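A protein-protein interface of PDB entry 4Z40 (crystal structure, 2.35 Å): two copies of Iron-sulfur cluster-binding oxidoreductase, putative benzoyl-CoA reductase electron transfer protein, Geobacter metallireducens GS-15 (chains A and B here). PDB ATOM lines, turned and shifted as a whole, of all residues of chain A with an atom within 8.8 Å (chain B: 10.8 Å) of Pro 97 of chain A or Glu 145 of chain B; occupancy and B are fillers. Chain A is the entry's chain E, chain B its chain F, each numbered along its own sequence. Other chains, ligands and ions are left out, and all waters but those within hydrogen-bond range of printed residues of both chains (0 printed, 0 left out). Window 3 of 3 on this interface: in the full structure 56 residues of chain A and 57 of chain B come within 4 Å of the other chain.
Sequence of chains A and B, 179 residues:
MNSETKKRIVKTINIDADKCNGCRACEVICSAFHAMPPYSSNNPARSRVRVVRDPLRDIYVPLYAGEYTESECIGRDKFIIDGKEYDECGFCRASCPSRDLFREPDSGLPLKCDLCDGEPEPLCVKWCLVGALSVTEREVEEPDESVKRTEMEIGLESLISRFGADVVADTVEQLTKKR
The side-chain carboxylate (OE2) of Glu 70 of chain A is in salt-bridge range of the guanidinium group (NE) of Arg 149 of chain B (2.9 Å).
OE2 of Glu 67 of chain B is in hydrogen-bond range of OG of Ser 71 of chain A (3.0 Å).
N of Glu 72 of chain A sits at hydrogen-bond distance from OG of Ser 146 of chain B, 2.7 Å away.
The side-chain carboxylate (OE2) of Glu 72 of chain A is in salt-bridge range of the guanidinium group (NH1) of Arg 8 of chain B (2.7 Å).
The backbone carbonyl oxygen of Glu 72 of chain A lies close to the side-chain carboxylate of Glu 67 of chain B.
O of Glu 70 of chain A is in hydrogen-bond range of N of Val 147 of chain B (3.0 Å).
OD2 of Asp 144 of chain B lies within salt-bridge range of NH1 of Arg 8 of chain B.
The backbone carbonyl oxygen (O) of Ser 95 of chain A sits at hydrogen-bond distance from the backbone NH (N) of Thr 69 of chain A, 3.0 Å away.
NE of Arg 8 of chain B is in hydrogen-bond range of O of Glu 142 of chain B, at 3.2 Å.
NH2 of Arg 8 of chain B is in hydrogen-bond range of O of Pro 143 of chain B (3.5 Å).
The backbone carbonyl oxygen of Arg 8 of chain B is in hydrogen-bond range of the backbone NH of Val 140 of chain B, 3.0 Å away.
OD1 of Asp 144 of chain B lies within hydrogen-bond range of N of Ser 146 of chain B (3.2 Å).
Thr 69 of chain A touches Glu 67 of chain B (OG1 to CB, 3.6 Å).
Ser 146 of chain B touches Glu 70 of chain A (CA to O, 3.6 Å).
Ser 71 of chain A touches Ser 146 of chain B (CA to OG, 3.3 Å).
Val 147 of chain B touches Ser 71 of chain A (O to CB, 3.7 Å).
CA of Cys 73 of chain A touches OE1 of Glu 67 of chain B, at 3.6 Å.
Arg 76 of chain A touches Arg 8 of chain B.
Arg 76 of chain A touches Val 10 of chain B.
O of Pro 97 of chain A touches OE1 of Glu 145 of chain B (3.6 Å).
Pro 97 of chain A touches one residue of chain B.
No residue of chain B comes within 4 Å of Cys 96 of chain A.
No residue of chain B comes within 4 Å of Ser 98 of chain A.
Of the printed residues of chain B, Glu 72 of chain A touches Arg 8, Glu 67 and Ser 146.
Of the printed residues of chain B, Glu 70 of chain A touches Ser 146 (3.6 Å), Val 147 (3.0 Å) and Arg 149 (2.9 Å).
Of the printed residues of chain A, Val 147 of chain B touches Glu 70 (3.0 Å) and Ser 71 (3.7 Å).
Of the printed residues of chain A, Arg 149 of chain B touches Glu 70.
Of the printed residues of chain B, Ser 71 of chain A touches Glu 67, Ser 146 and Val 147.
Leu 101 of chain A touches none of the printed residues of chain B.
The nearest printed residue of chain A that does not touch Val 147 of chain B is Tyr 68 of chain A (5.5 Å).
Of the 15 printed residues of chain B, 7 touch a printed residue of chain A.
Hydrophobic or aromatic side chains of chain B within 4 Å of the printed part of chain A: Val 10 and Val 147.
Among the printed residues, 14 pairs touch across the chains.
Positions printed for both chains: 67 and 68.
Of the 14 pairs that touch across the chains among the printed residues, none has its exchanged pair printed and touching as well.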
ATOM      1  N   GLU A  67       2.991  31.748  24.748  1.00  0.00           N
ATOM      2  CA  GLU A  67       1.648  31.216  24.704  1.00  0.00           C
ATOM      3  C   GLU A  67       1.547  29.937  23.885  1.00  0.00           C
ATOM      4  O   GLU A  67       2.480  29.572  23.157  1.00  0.00           O
ATOM      5  CB  GLU A  67       0.695  32.274  24.151  1.00  0.00           C
ATOM      6  CG  GLU A  67       0.341  33.316  25.170  1.00  0.00           C
ATOM      7  CD  GLU A  67      -0.346  32.705  26.376  1.00  0.00           C
ATOM      8  OE1 GLU A  67      -0.995  31.646  26.223  1.00  0.00           O
ATOM      9  OE2 GLU A  67      -0.235  33.277  27.479  1.00  0.00           O
ATOM     10  N   TYR A  68       0.406  29.261  24.009  1.00  0.00           N
ATOM     11  CA  TYR A  68       0.147  28.068  23.216  1.00  0.00           C
ATOM     12  C   TYR A  68      -0.602  28.395  21.924  1.00  0.00           C
ATOM     13  O   TYR A  68      -1.645  29.055  21.943  1.00  0.00           O
ATOM     14  CB  TYR A  68      -0.645  27.041  24.030  1.00  0.00           C
ATOM     15  CG  TYR A  68      -1.296  25.977  23.171  1.00  0.00           C
ATOM     16  CD1 TYR A  68      -0.552  24.918  22.636  1.00  0.00           C
ATOM     17  CD2 TYR A  68      -2.652  26.036  22.884  1.00  0.00           C
ATOM     18  CE1 TYR A  68      -1.155  23.947  21.842  1.00  0.00           C
ATOM     19  CE2 TYR A  68      -3.263  25.081  22.093  1.00  0.00           C
ATOM     20  CZ  TYR A  68      -2.520  24.043  21.572  1.00  0.00           C
ATOM     21  OH  TYR A  68      -3.164  23.114  20.790  1.00  0.00           O
ATOM     22  N   THR A  69      -0.069  27.921  20.803  1.00  0.00           N
ATOM     23  CA  THR A  69      -0.750  28.028  19.517  1.00  0.00           C
ATOM     24  C   THR A  69      -0.988  26.636  18.927  1.00  0.00           C
ATOM     25  O   THR A  69      -0.122  25.757  19.021  1.00  0.00           O
ATOM     26  CB  THR A  69       0.058  28.878  18.515  1.00  0.00           C
ATOM     27  OG1 THR A  69      -0.517  28.761  17.213  1.00  0.00           O
ATOM     28  CG2 THR A  69       1.487  28.393  18.441  1.00  0.00           C
ATOM     29  N   GLU A  70      -2.149  26.445  18.305  1.00  0.00           N
ATOM     30  CA  GLU A  70      -2.553  25.147  17.778  1.00  0.00           C
ATOM     31  C   GLU A  70      -2.070  24.903  16.347  1.00  0.00           C
ATOM     32  O   GLU A  70      -2.141  23.779  15.844  1.00  0.00           O
ATOM     33  CB  GLU A  70      -4.072  25.026  17.807  1.00  0.00           C
ATOM     34  CG  GLU A  70      -4.722  25.962  16.808  1.00  0.00           C
ATOM     35  CD  GLU A  70      -6.238  25.909  16.809  1.00  0.00           C
ATOM     36  OE1 GLU A  70      -6.832  25.252  17.695  1.00  0.00           O
ATOM     37  OE2 GLU A  70      -6.832  26.537  15.907  1.00  0.00           O
ATOM     38  N   SER A  71      -1.604  25.954  15.684  1.00  0.00           N
ATOM     39  CA  SER A  71      -1.201  25.837  14.294  1.00  0.00           C
ATOM     40  C   SER A  71       0.039  26.662  14.039  1.00  0.00           C
ATOM     41  O   SER A  71       0.269  27.667  14.710  1.00  0.00           O
ATOM     42  CB  SER A  71      -2.337  26.284  13.361  1.00  0.00           C
ATOM     43  OG  SER A  71      -2.685  27.641  13.568  1.00  0.00           O
ATOM     44  N   GLU A  72       0.845  26.227  13.075  1.00  0.00           N
ATOM     45  CA  GLU A  72       2.038  26.964  12.667  1.00  0.00           C
ATOM     46  C   GLU A  72       1.619  28.189  11.873  1.00  0.00           C
ATOM     47  O   GLU A  72       0.466  28.303  11.445  1.00  0.00           O
ATOM     48  CB  GLU A  72       2.975  26.096  11.810  1.00  0.00           C
ATOM     49  CG  GLU A  72       3.461  24.795  12.449  1.00  0.00           C
ATOM     50  CD  GLU A  72       4.207  23.902  11.454  1.00  0.00           C
ATOM     51  OE1 GLU A  72       4.470  22.723  11.782  1.00  0.00           O
ATOM     52  OE2 GLU A  72       4.523  24.377  10.340  1.00  0.00           O
ATOM     53  N   CYS A  73       2.558  29.101  11.670  1.00  0.00           N
ATOM     54  CA  CYS A  73       2.307  30.244  10.818  1.00  0.00           C
ATOM     55  C   CYS A  73       2.374  29.821   9.362  1.00  0.00           C
ATOM     56  O   CYS A  73       3.113  28.893   9.017  1.00  0.00           O
ATOM     57  CB  CYS A  73       3.316  31.350  11.093  1.00  0.00           C
ATOM     58  SG  CYS A  73       3.151  32.093  12.736  1.00  0.00           S
ATOM     59  N   ARG A  76       7.127  31.280   8.056  1.00  0.00           N
ATOM     60  CA  ARG A  76       8.063  31.415   9.171  1.00  0.00           C
ATOM     61  C   ARG A  76       9.014  32.572   8.918  1.00  0.00           C
ATOM     62  O   ARG A  76       9.306  32.866   7.759  1.00  0.00           O
ATOM     63  CB  ARG A  76       8.850  30.130   9.359  1.00  0.00           C
ATOM     64  CG  ARG A  76       7.980  28.951   9.645  1.00  0.00           C
ATOM     65  CD  ARG A  76       8.788  27.705   9.709  1.00  0.00           C
ATOM     66  NE  ARG A  76       7.917  26.568   9.951  1.00  0.00           N
ATOM     67  CZ  ARG A  76       8.340  25.338  10.207  1.00  0.00           C
ATOM     68  NH1 ARG A  76       9.641  25.072  10.263  1.00  0.00           N
ATOM     69  NH2 ARG A  76       7.453  24.377  10.410  1.00  0.00           N
ATOM     70  N   ALA A  94       6.514  30.998  21.346  1.00  0.00           N
ATOM     71  CA  ALA A  94       5.302  30.176  21.284  1.00  0.00           C
ATOM     72  C   ALA A  94       5.538  28.690  21.555  1.00  0.00           C
ATOM     73  O   ALA A  94       6.556  28.108  21.163  1.00  0.00           O
ATOM     74  CB  ALA A  94       4.618  30.345  19.930  1.00  0.00           C
ATOM     75  N   SER A  95       4.579  28.079  22.238  1.00  0.00           N
ATOM     76  CA  SER A  95       4.478  26.634  22.253  1.00  0.00           C
ATOM     77  C   SER A  95       3.694  26.249  20.990  1.00  0.00           C
ATOM     78  O   SER A  95       2.461  26.246  20.984  1.00  0.00           O
ATOM     79  CB  SER A  95       3.799  26.139  23.527  1.00  0.00           C
ATOM     80  OG  SER A  95       3.742  24.725  23.545  1.00  0.00           O
ATOM     81  N   CYS A  96       4.446  25.937  19.932  1.00  0.00           N
ATOM     82  CA  CYS A  96       3.960  25.801  18.565  1.00  0.00           C
ATOM     83  C   CYS A  96       4.258  24.406  18.011  1.00  0.00           C
ATOM     84  O   CYS A  96       5.283  23.813  18.344  1.00  0.00           O
ATOM     85  CB  CYS A  96       4.602  26.889  17.687  1.00  0.00           C
ATOM     86  SG  CYS A  96       4.497  26.696  15.877  1.00  0.00           S
ATOM     87  N   PRO A  97       3.354  23.868  17.169  1.00  0.00           N
ATOM     88  CA  PRO A  97       3.508  22.507  16.625  1.00  0.00           C
ATOM     89  C   PRO A  97       4.745  22.282  15.740  1.00  0.00           C
ATOM     90  O   PRO A  97       5.064  21.133  15.446  1.00  0.00           O
ATOM     91  CB  PRO A  97       2.223  22.307  15.806  1.00  0.00           C
ATOM     92  CG  PRO A  97       1.648  23.679  15.609  1.00  0.00           C
ATOM     93  CD  PRO A  97       2.052  24.457  16.819  1.00  0.00           C
ATOM     94  N   SER A  98       5.434  23.346  15.345  1.00  0.00           N
ATOM     95  CA  SER A  98       6.603  23.245  14.464  1.00  0.00           C
ATOM     96  C   SER A  98       7.916  22.824  15.166  1.00  0.00           C
ATOM     97  O   SER A  98       8.916  22.535  14.514  1.00  0.00           O
ATOM     98  CB  SER A  98       6.826  24.591  13.765  1.00  0.00           C
ATOM     99  OG  SER A  98       7.059  25.625  14.717  1.00  0.00           O
ATOM    100  N   ARG A  99       7.932  22.806  16.489  1.00  0.00           N
ATOM    101  CA  ARG A  99       9.181  22.554  17.191  1.00  0.00           C
ATOM    102  C   ARG A  99       8.902  21.984  18.566  1.00  0.00           C
ATOM    103  O   ARG A  99       7.736  21.880  18.983  1.00  0.00           O
ATOM    104  CB  ARG A  99       9.991  23.844  17.311  1.00  0.00           C
ATOM    105  CG  ARG A  99       9.130  24.959  17.838  1.00  0.00           C
ATOM    106  CD  ARG A  99       9.809  26.294  17.878  1.00  0.00           C
ATOM    107  NE  ARG A  99       9.028  27.171  18.739  1.00  0.00           N
ATOM    108  CZ  ARG A  99       9.452  28.344  19.187  1.00  0.00           C
ATOM    109  NH1 ARG A  99      10.663  28.784  18.856  1.00  0.00           N
ATOM    110  NH2 ARG A  99       8.678  29.068  19.982  1.00  0.00           N
ATOM    111  N   ASP A 100       9.980  21.632  19.266  1.00  0.00           N
ATOM    112  CA  ASP A 100       9.880  21.000  20.573  1.00  0.00           C
ATOM    113  C   ASP A 100      10.103  21.962  21.734  1.00  0.00           C
ATOM    114  O   ASP A 100       9.797  21.619  22.878  1.00  0.00           O
ATOM    115  CB  ASP A 100      10.874  19.850  20.670  1.00  0.00           C
ATOM    116  CG  ASP A 100      10.599  18.771  19.658  1.00  0.00           C
ATOM    117  OD1 ASP A 100       9.408  18.614  19.291  1.00  0.00           O
ATOM    118  OD2 ASP A 100      11.563  18.091  19.229  1.00  0.00           O
ATOM    119  N   LEU A 101      10.647  23.146  21.450  1.00  0.00           N
ATOM    120  CA  LEU A 101      10.786  24.182  22.470  1.00  0.00           C
ATOM    121  C   LEU A 101       9.494  24.361  23.259  1.00  0.00           C
ATOM    122  O   LEU A 101       8.406  24.325  22.695  1.00  0.00           O
ATOM    123  CB  LEU A 101      11.162  25.522  21.850  1.00  0.00           C
ATOM    124  CG  LEU A 101      12.577  25.863  21.395  1.00  0.00           C
ATOM    125  CD1 LEU A 101      12.657  27.369  21.176  1.00  0.00           C
ATOM    126  CD2 LEU A 101      13.645  25.399  22.385  1.00  0.00           C
ATOM    127  N   ARG A 103       7.748  22.591  25.032  1.00  0.00           N
ATOM    128  CA  ARG A 103       6.831  21.455  25.030  1.00  0.00           C
ATOM    129  C   ARG A 103       7.483  20.236  25.681  1.00  0.00           C
ATOM    130  O   ARG A 103       8.664  19.973  25.447  1.00  0.00           O
ATOM    131  CB  ARG A 103       6.407  21.118  23.607  1.00  0.00           C
ATOM    132  CG  ARG A 103       5.775  22.281  22.866  1.00  0.00           C
ATOM    133  CD  ARG A 103       5.549  21.945  21.414  1.00  0.00           C
ATOM    134  NE  ARG A 103       4.640  20.819  21.256  1.00  0.00           N
ATOM    135  CZ  ARG A 103       4.650  20.016  20.201  1.00  0.00           C
ATOM    136  NH1 ARG A 103       5.535  20.219  19.233  1.00  0.00           N
ATOM    137  NH2 ARG A 103       3.787  19.011  20.115  1.00  0.00           N
ATOM    138  N   SER A 107       5.535  13.742  26.350  1.00  0.00           N
ATOM    139  CA  SER A 107       4.158  13.860  25.861  1.00  0.00           C
ATOM    140  C   SER A 107       4.015  14.875  24.728  1.00  0.00           C
ATOM    141  O   SER A 107       3.547  14.533  23.644  1.00  0.00           O
ATOM    142  CB  SER A 107       3.211  14.219  27.009  1.00  0.00           C
ATOM    143  OG  SER A 107       3.532  15.471  27.571  1.00  0.00           O
ATOM    144  N   GLY A 108       4.420  16.116  24.970  1.00  0.00           N
ATOM    145  CA  GLY A 108       4.339  17.145  23.949  1.00  0.00           C
ATOM    146  C   GLY A 108       3.443  18.287  24.390  1.00  0.00           C
ATOM    147  O   GLY A 108       3.194  19.234  23.637  1.00  0.00           O
ATOM    148  N   ARG B   8       5.895  17.810   3.144  1.00  0.00           N
ATOM    149  CA  ARG B   8       5.168  19.056   2.904  1.00  0.00           C
ATOM    150  C   ARG B   8       6.082  20.230   2.575  1.00  0.00           C
ATOM    151  O   ARG B   8       7.292  20.077   2.479  1.00  0.00           O
ATOM    152  CB  ARG B   8       4.320  19.421   4.120  1.00  0.00           C
ATOM    153  CG  ARG B   8       5.106  19.441   5.412  1.00  0.00           C
ATOM    154  CD  ARG B   8       4.662  20.552   6.355  1.00  0.00           C
ATOM    155  NE  ARG B   8       5.198  20.355   7.702  1.00  0.00           N
ATOM    156  CZ  ARG B   8       5.020  21.205   8.711  1.00  0.00           C
ATOM    157  NH1 ARG B   8       4.323  22.324   8.524  1.00  0.00           N
ATOM    158  NH2 ARG B   8       5.540  20.940   9.906  1.00  0.00           N
ATOM    159  N   ILE B   9       5.487  21.408   2.413  1.00  0.00           N
ATOM    160  CA  ILE B   9       6.243  22.625   2.130  1.00  0.00           C
ATOM    161  C   ILE B   9       6.082  23.691   3.217  1.00  0.00           C
ATOM    162  O   ILE B   9       4.967  24.084   3.553  1.00  0.00           O
ATOM    163  CB  ILE B   9       5.827  23.242   0.796  1.00  0.00           C
ATOM    164  CG1 ILE B   9       6.166  22.299  -0.353  1.00  0.00           C
ATOM    165  CG2 ILE B   9       6.504  24.594   0.599  1.00  0.00           C
ATOM    166  CD1 ILE B   9       5.747  22.837  -1.699  1.00  0.00           C
ATOM    167  N   VAL B  10       7.204  24.146   3.769  1.00  0.00           N
ATOM    168  CA  VAL B  10       7.197  25.279   4.683  1.00  0.00           C
ATOM    169  C   VAL B  10       7.858  26.463   3.995  1.00  0.00           C
ATOM    170  O   VAL B  10       8.797  26.303   3.204  1.00  0.00           O
ATOM    171  CB  VAL B  10       7.908  24.966   6.037  1.00  0.00           C
ATOM    172  CG1 VAL B  10       8.346  23.540   6.085  1.00  0.00           C
ATOM    173  CG2 VAL B  10       9.072  25.922   6.305  1.00  0.00           C
ATOM    174  N   GLU B  67       0.180  34.245  14.855  1.00  0.00           N
ATOM    175  CA  GLU B  67      -0.992  33.504  15.293  1.00  0.00           C
ATOM    176  C   GLU B  67      -1.684  34.207  16.450  1.00  0.00           C
ATOM    177  O   GLU B  67      -1.084  34.991  17.194  1.00  0.00           O
ATOM    178  CB  GLU B  67      -0.621  32.070  15.689  1.00  0.00           C
ATOM    179  CG  GLU B  67      -0.072  31.227  14.539  1.00  0.00           C
ATOM    180  CD  GLU B  67      -1.075  31.073  13.414  1.00  0.00           C
ATOM    181  OE1 GLU B  67      -0.729  31.416  12.261  1.00  0.00           O
ATOM    182  OE2 GLU B  67      -2.208  30.613  13.684  1.00  0.00           O
ATOM    183  N   TYR B  68      -2.973  33.936  16.567  1.00  0.00           N
ATOM    184  CA  TYR B  68      -3.810  34.585  17.554  1.00  0.00           C
ATOM    185  C   TYR B  68      -3.590  33.995  18.942  1.00  0.00           C
ATOM    186  O   TYR B  68      -3.519  32.787  19.108  1.00  0.00           O
ATOM    187  CB  TYR B  68      -5.277  34.460  17.120  1.00  0.00           C
ATOM    188  CG  TYR B  68      -6.283  34.700  18.201  1.00  0.00           C
ATOM    189  CD1 TYR B  68      -6.676  35.984  18.537  1.00  0.00           C
ATOM    190  CD2 TYR B  68      -6.852  33.637  18.885  1.00  0.00           C
ATOM    191  CE1 TYR B  68      -7.608  36.207  19.536  1.00  0.00           C
ATOM    192  CE2 TYR B  68      -7.781  33.847  19.889  1.00  0.00           C
ATOM    193  CZ  TYR B  68      -8.161  35.133  20.207  1.00  0.00           C
ATOM    194  OH  TYR B  68      -9.095  35.335  21.198  1.00  0.00           O
ATOM    195  N   VAL B 140       9.954  19.408   3.740  1.00  0.00           N
ATOM    196  CA  VAL B 140      10.314  18.773   5.008  1.00  0.00           C
ATOM    197  C   VAL B 140       9.584  17.436   5.160  1.00  0.00           C
ATOM    198  O   VAL B 140       8.454  17.277   4.686  1.00  0.00           O
ATOM    199  CB  VAL B 140       9.989  19.684   6.224  1.00  0.00           C
ATOM    200  CG1 VAL B 140      10.841  20.948   6.204  1.00  0.00           C
ATOM    201  CG2 VAL B 140       8.513  20.037   6.242  1.00  0.00           C
ATOM    202  N   GLU B 141      10.235  16.475   5.806  1.00  0.00           N
ATOM    203  CA  GLU B 141       9.630  15.169   6.026  1.00  0.00           C
ATOM    204  C   GLU B 141       8.592  15.238   7.134  1.00  0.00           C
ATOM    205  O   GLU B 141       7.601  14.506   7.117  1.00  0.00           O
ATOM    206  CB  GLU B 141      10.699  14.133   6.376  1.00  0.00           C
ATOM    207  CG  GLU B 141      11.632  14.566   7.500  1.00  0.00           C
ATOM    208  CD  GLU B 141      12.286  13.394   8.206  1.00  0.00           C
ATOM    209  OE1 GLU B 141      11.651  12.320   8.287  1.00  0.00           O
ATOM    210  OE2 GLU B 141      13.434  13.547   8.681  1.00  0.00           O
ATOM    211  N   GLU B 142       8.837  16.129   8.092  1.00  0.00           N
ATOM    212  CA  GLU B 142       8.003  16.263   9.283  1.00  0.00           C
ATOM    213  C   GLU B 142       6.537  16.484   8.941  1.00  0.00           C
ATOM    214  O   GLU B 142       6.207  17.345   8.126  1.00  0.00           O
ATOM    215  CB  GLU B 142       8.501  17.417  10.159  1.00  0.00           C
ATOM    216  CG  GLU B 142       9.871  17.200  10.794  1.00  0.00           C
ATOM    217  CD  GLU B 142      11.024  17.654   9.910  1.00  0.00           C
ATOM    218  OE1 GLU B 142      12.045  18.116  10.460  1.00  0.00           O
ATOM    219  OE2 GLU B 142      10.915  17.547   8.671  1.00  0.00           O
ATOM    220  N   PRO B 143       5.653  15.692   9.565  1.00  0.00           N
ATOM    221  CA  PRO B 143       4.202  15.838   9.403  1.00  0.00           C
ATOM    222  C   PRO B 143       3.710  17.225   9.828  1.00  0.00           C
ATOM    223  O   PRO B 143       4.290  17.824  10.734  1.00  0.00           O
ATOM    224  CB  PRO B 143       3.638  14.751  10.324  1.00  0.00           C
ATOM    225  CG  PRO B 143       4.742  13.748  10.455  1.00  0.00           C
ATOM    226  CD  PRO B 143       6.006  14.546  10.421  1.00  0.00           C
ATOM    227  N   ASP B 144       2.664  17.726   9.176  1.00  0.00           N
ATOM    228  CA  ASP B 144       2.054  18.999   9.563  1.00  0.00           C
ATOM    229  C   ASP B 144       0.938  18.753  10.573  1.00  0.00           C
ATOM    230  O   ASP B 144      -0.118  18.227  10.221  1.00  0.00           O
ATOM    231  CB  ASP B 144       1.508  19.741   8.336  1.00  0.00           C
ATOM    232  CG  ASP B 144       1.195  21.207   8.621  1.00  0.00           C
ATOM    233  OD1 ASP B 144       1.134  21.593   9.809  1.00  0.00           O
ATOM    234  OD2 ASP B 144       1.005  21.976   7.651  1.00  0.00           O
ATOM    235  N   GLU B 145       1.168  19.146  11.823  1.00  0.00           N
ATOM    236  CA  GLU B 145       0.215  18.870  12.898  1.00  0.00           C
ATOM    237  C   GLU B 145      -0.669  20.073  13.254  1.00  0.00           C
ATOM    238  O   GLU B 145      -1.313  20.092  14.305  1.00  0.00           O
ATOM    239  CB  GLU B 145       0.968  18.392  14.139  1.00  0.00           C
ATOM    240  CG  GLU B 145       1.799  17.145  13.903  1.00  0.00           C
ATOM    241  CD  GLU B 145       2.935  17.009  14.901  1.00  0.00           C
ATOM    242  OE1 GLU B 145       3.238  18.006  15.596  1.00  0.00           O
ATOM    243  OE2 GLU B 145       3.526  15.909  14.991  1.00  0.00           O
ATOM    244  N   SER B 146      -0.702  21.071  12.376  1.00  0.00           N
ATOM    245  CA  SER B 146      -1.494  22.270  12.619  1.00  0.00           C
ATOM    246  C   SER B 146      -2.993  21.988  12.604  1.00  0.00           C
ATOM    247  O   SER B 146      -3.490  21.256  11.748  1.00  0.00           O
ATOM    248  CB  SER B 146      -1.173  23.344  11.581  1.00  0.00           C
ATOM    249  OG  SER B 146       0.058  23.973  11.858  1.00  0.00           O
ATOM    250  N   VAL B 147      -3.707  22.568  13.563  1.00  0.00           N
ATOM    251  CA  VAL B 147      -5.159  22.596  13.520  1.00  0.00           C
ATOM    252  C   VAL B 147      -5.574  23.725  12.585  1.00  0.00           C
ATOM    253  O   VAL B 147      -5.741  24.869  13.012  1.00  0.00           O
ATOM    254  CB  VAL B 147      -5.773  22.801  14.918  1.00  0.00           C
ATOM    255  CG1 VAL B 147      -7.295  22.803  14.844  1.00  0.00           C
ATOM    256  CG2 VAL B 147      -5.286  21.722  15.872  1.00  0.00           C
ATOM    257  N   LYS B 148      -5.714  23.409  11.301  1.00  0.00           N
ATOM    258  CA  LYS B 148      -5.988  24.433  10.301  1.00  0.00           C
ATOM    259  C   LYS B 148      -7.376  25.023  10.481  1.00  0.00           C
ATOM    260  O   LYS B 148      -8.382  24.374  10.203  1.00  0.00           O
ATOM    261  CB  LYS B 148      -5.834  23.868   8.891  1.00  0.00           C
ATOM    262  CG  LYS B 148      -4.391  23.603   8.490  1.00  0.00           C
ATOM    263  CD  LYS B 148      -4.268  23.444   6.986  1.00  0.00           C
ATOM    264  CE  LYS B 148      -4.814  24.670   6.263  1.00  0.00           C
ATOM    265  NZ  LYS B 148      -4.086  25.916   6.639  1.00  0.00           N
ATOM    266  N   ARG B 149      -7.415  26.263  10.949  1.00  0.00           N
ATOM    267  CA  ARG B 149      -8.670  26.940  11.224  1.00  0.00           C
ATOM    268  C   ARG B 149      -8.852  28.118  10.267  1.00  0.00           C
ATOM    269  O   ARG B 149      -7.886  28.823   9.953  1.00  0.00           O
ATOM    270  CB  ARG B 149      -8.703  27.400  12.681  1.00  0.00           C
ATOM    271  CG  ARG B 149     -10.078  27.780  13.187  1.00  0.00           C
ATOM    272  CD  ARG B 149     -10.084  27.896  14.704  1.00  0.00           C
ATOM    273  NE  ARG B 149      -9.672  26.651  15.352  1.00  0.00           N
ATOM    274  CZ  ARG B 149     -10.512  25.698  15.753  1.00  0.00           C
ATOM    275  NH1 ARG B 149     -11.820  25.845  15.569  1.00  0.00           N
ATOM    276  NH2 ARG B 149     -10.046  24.599  16.336  1.00  0.00           N
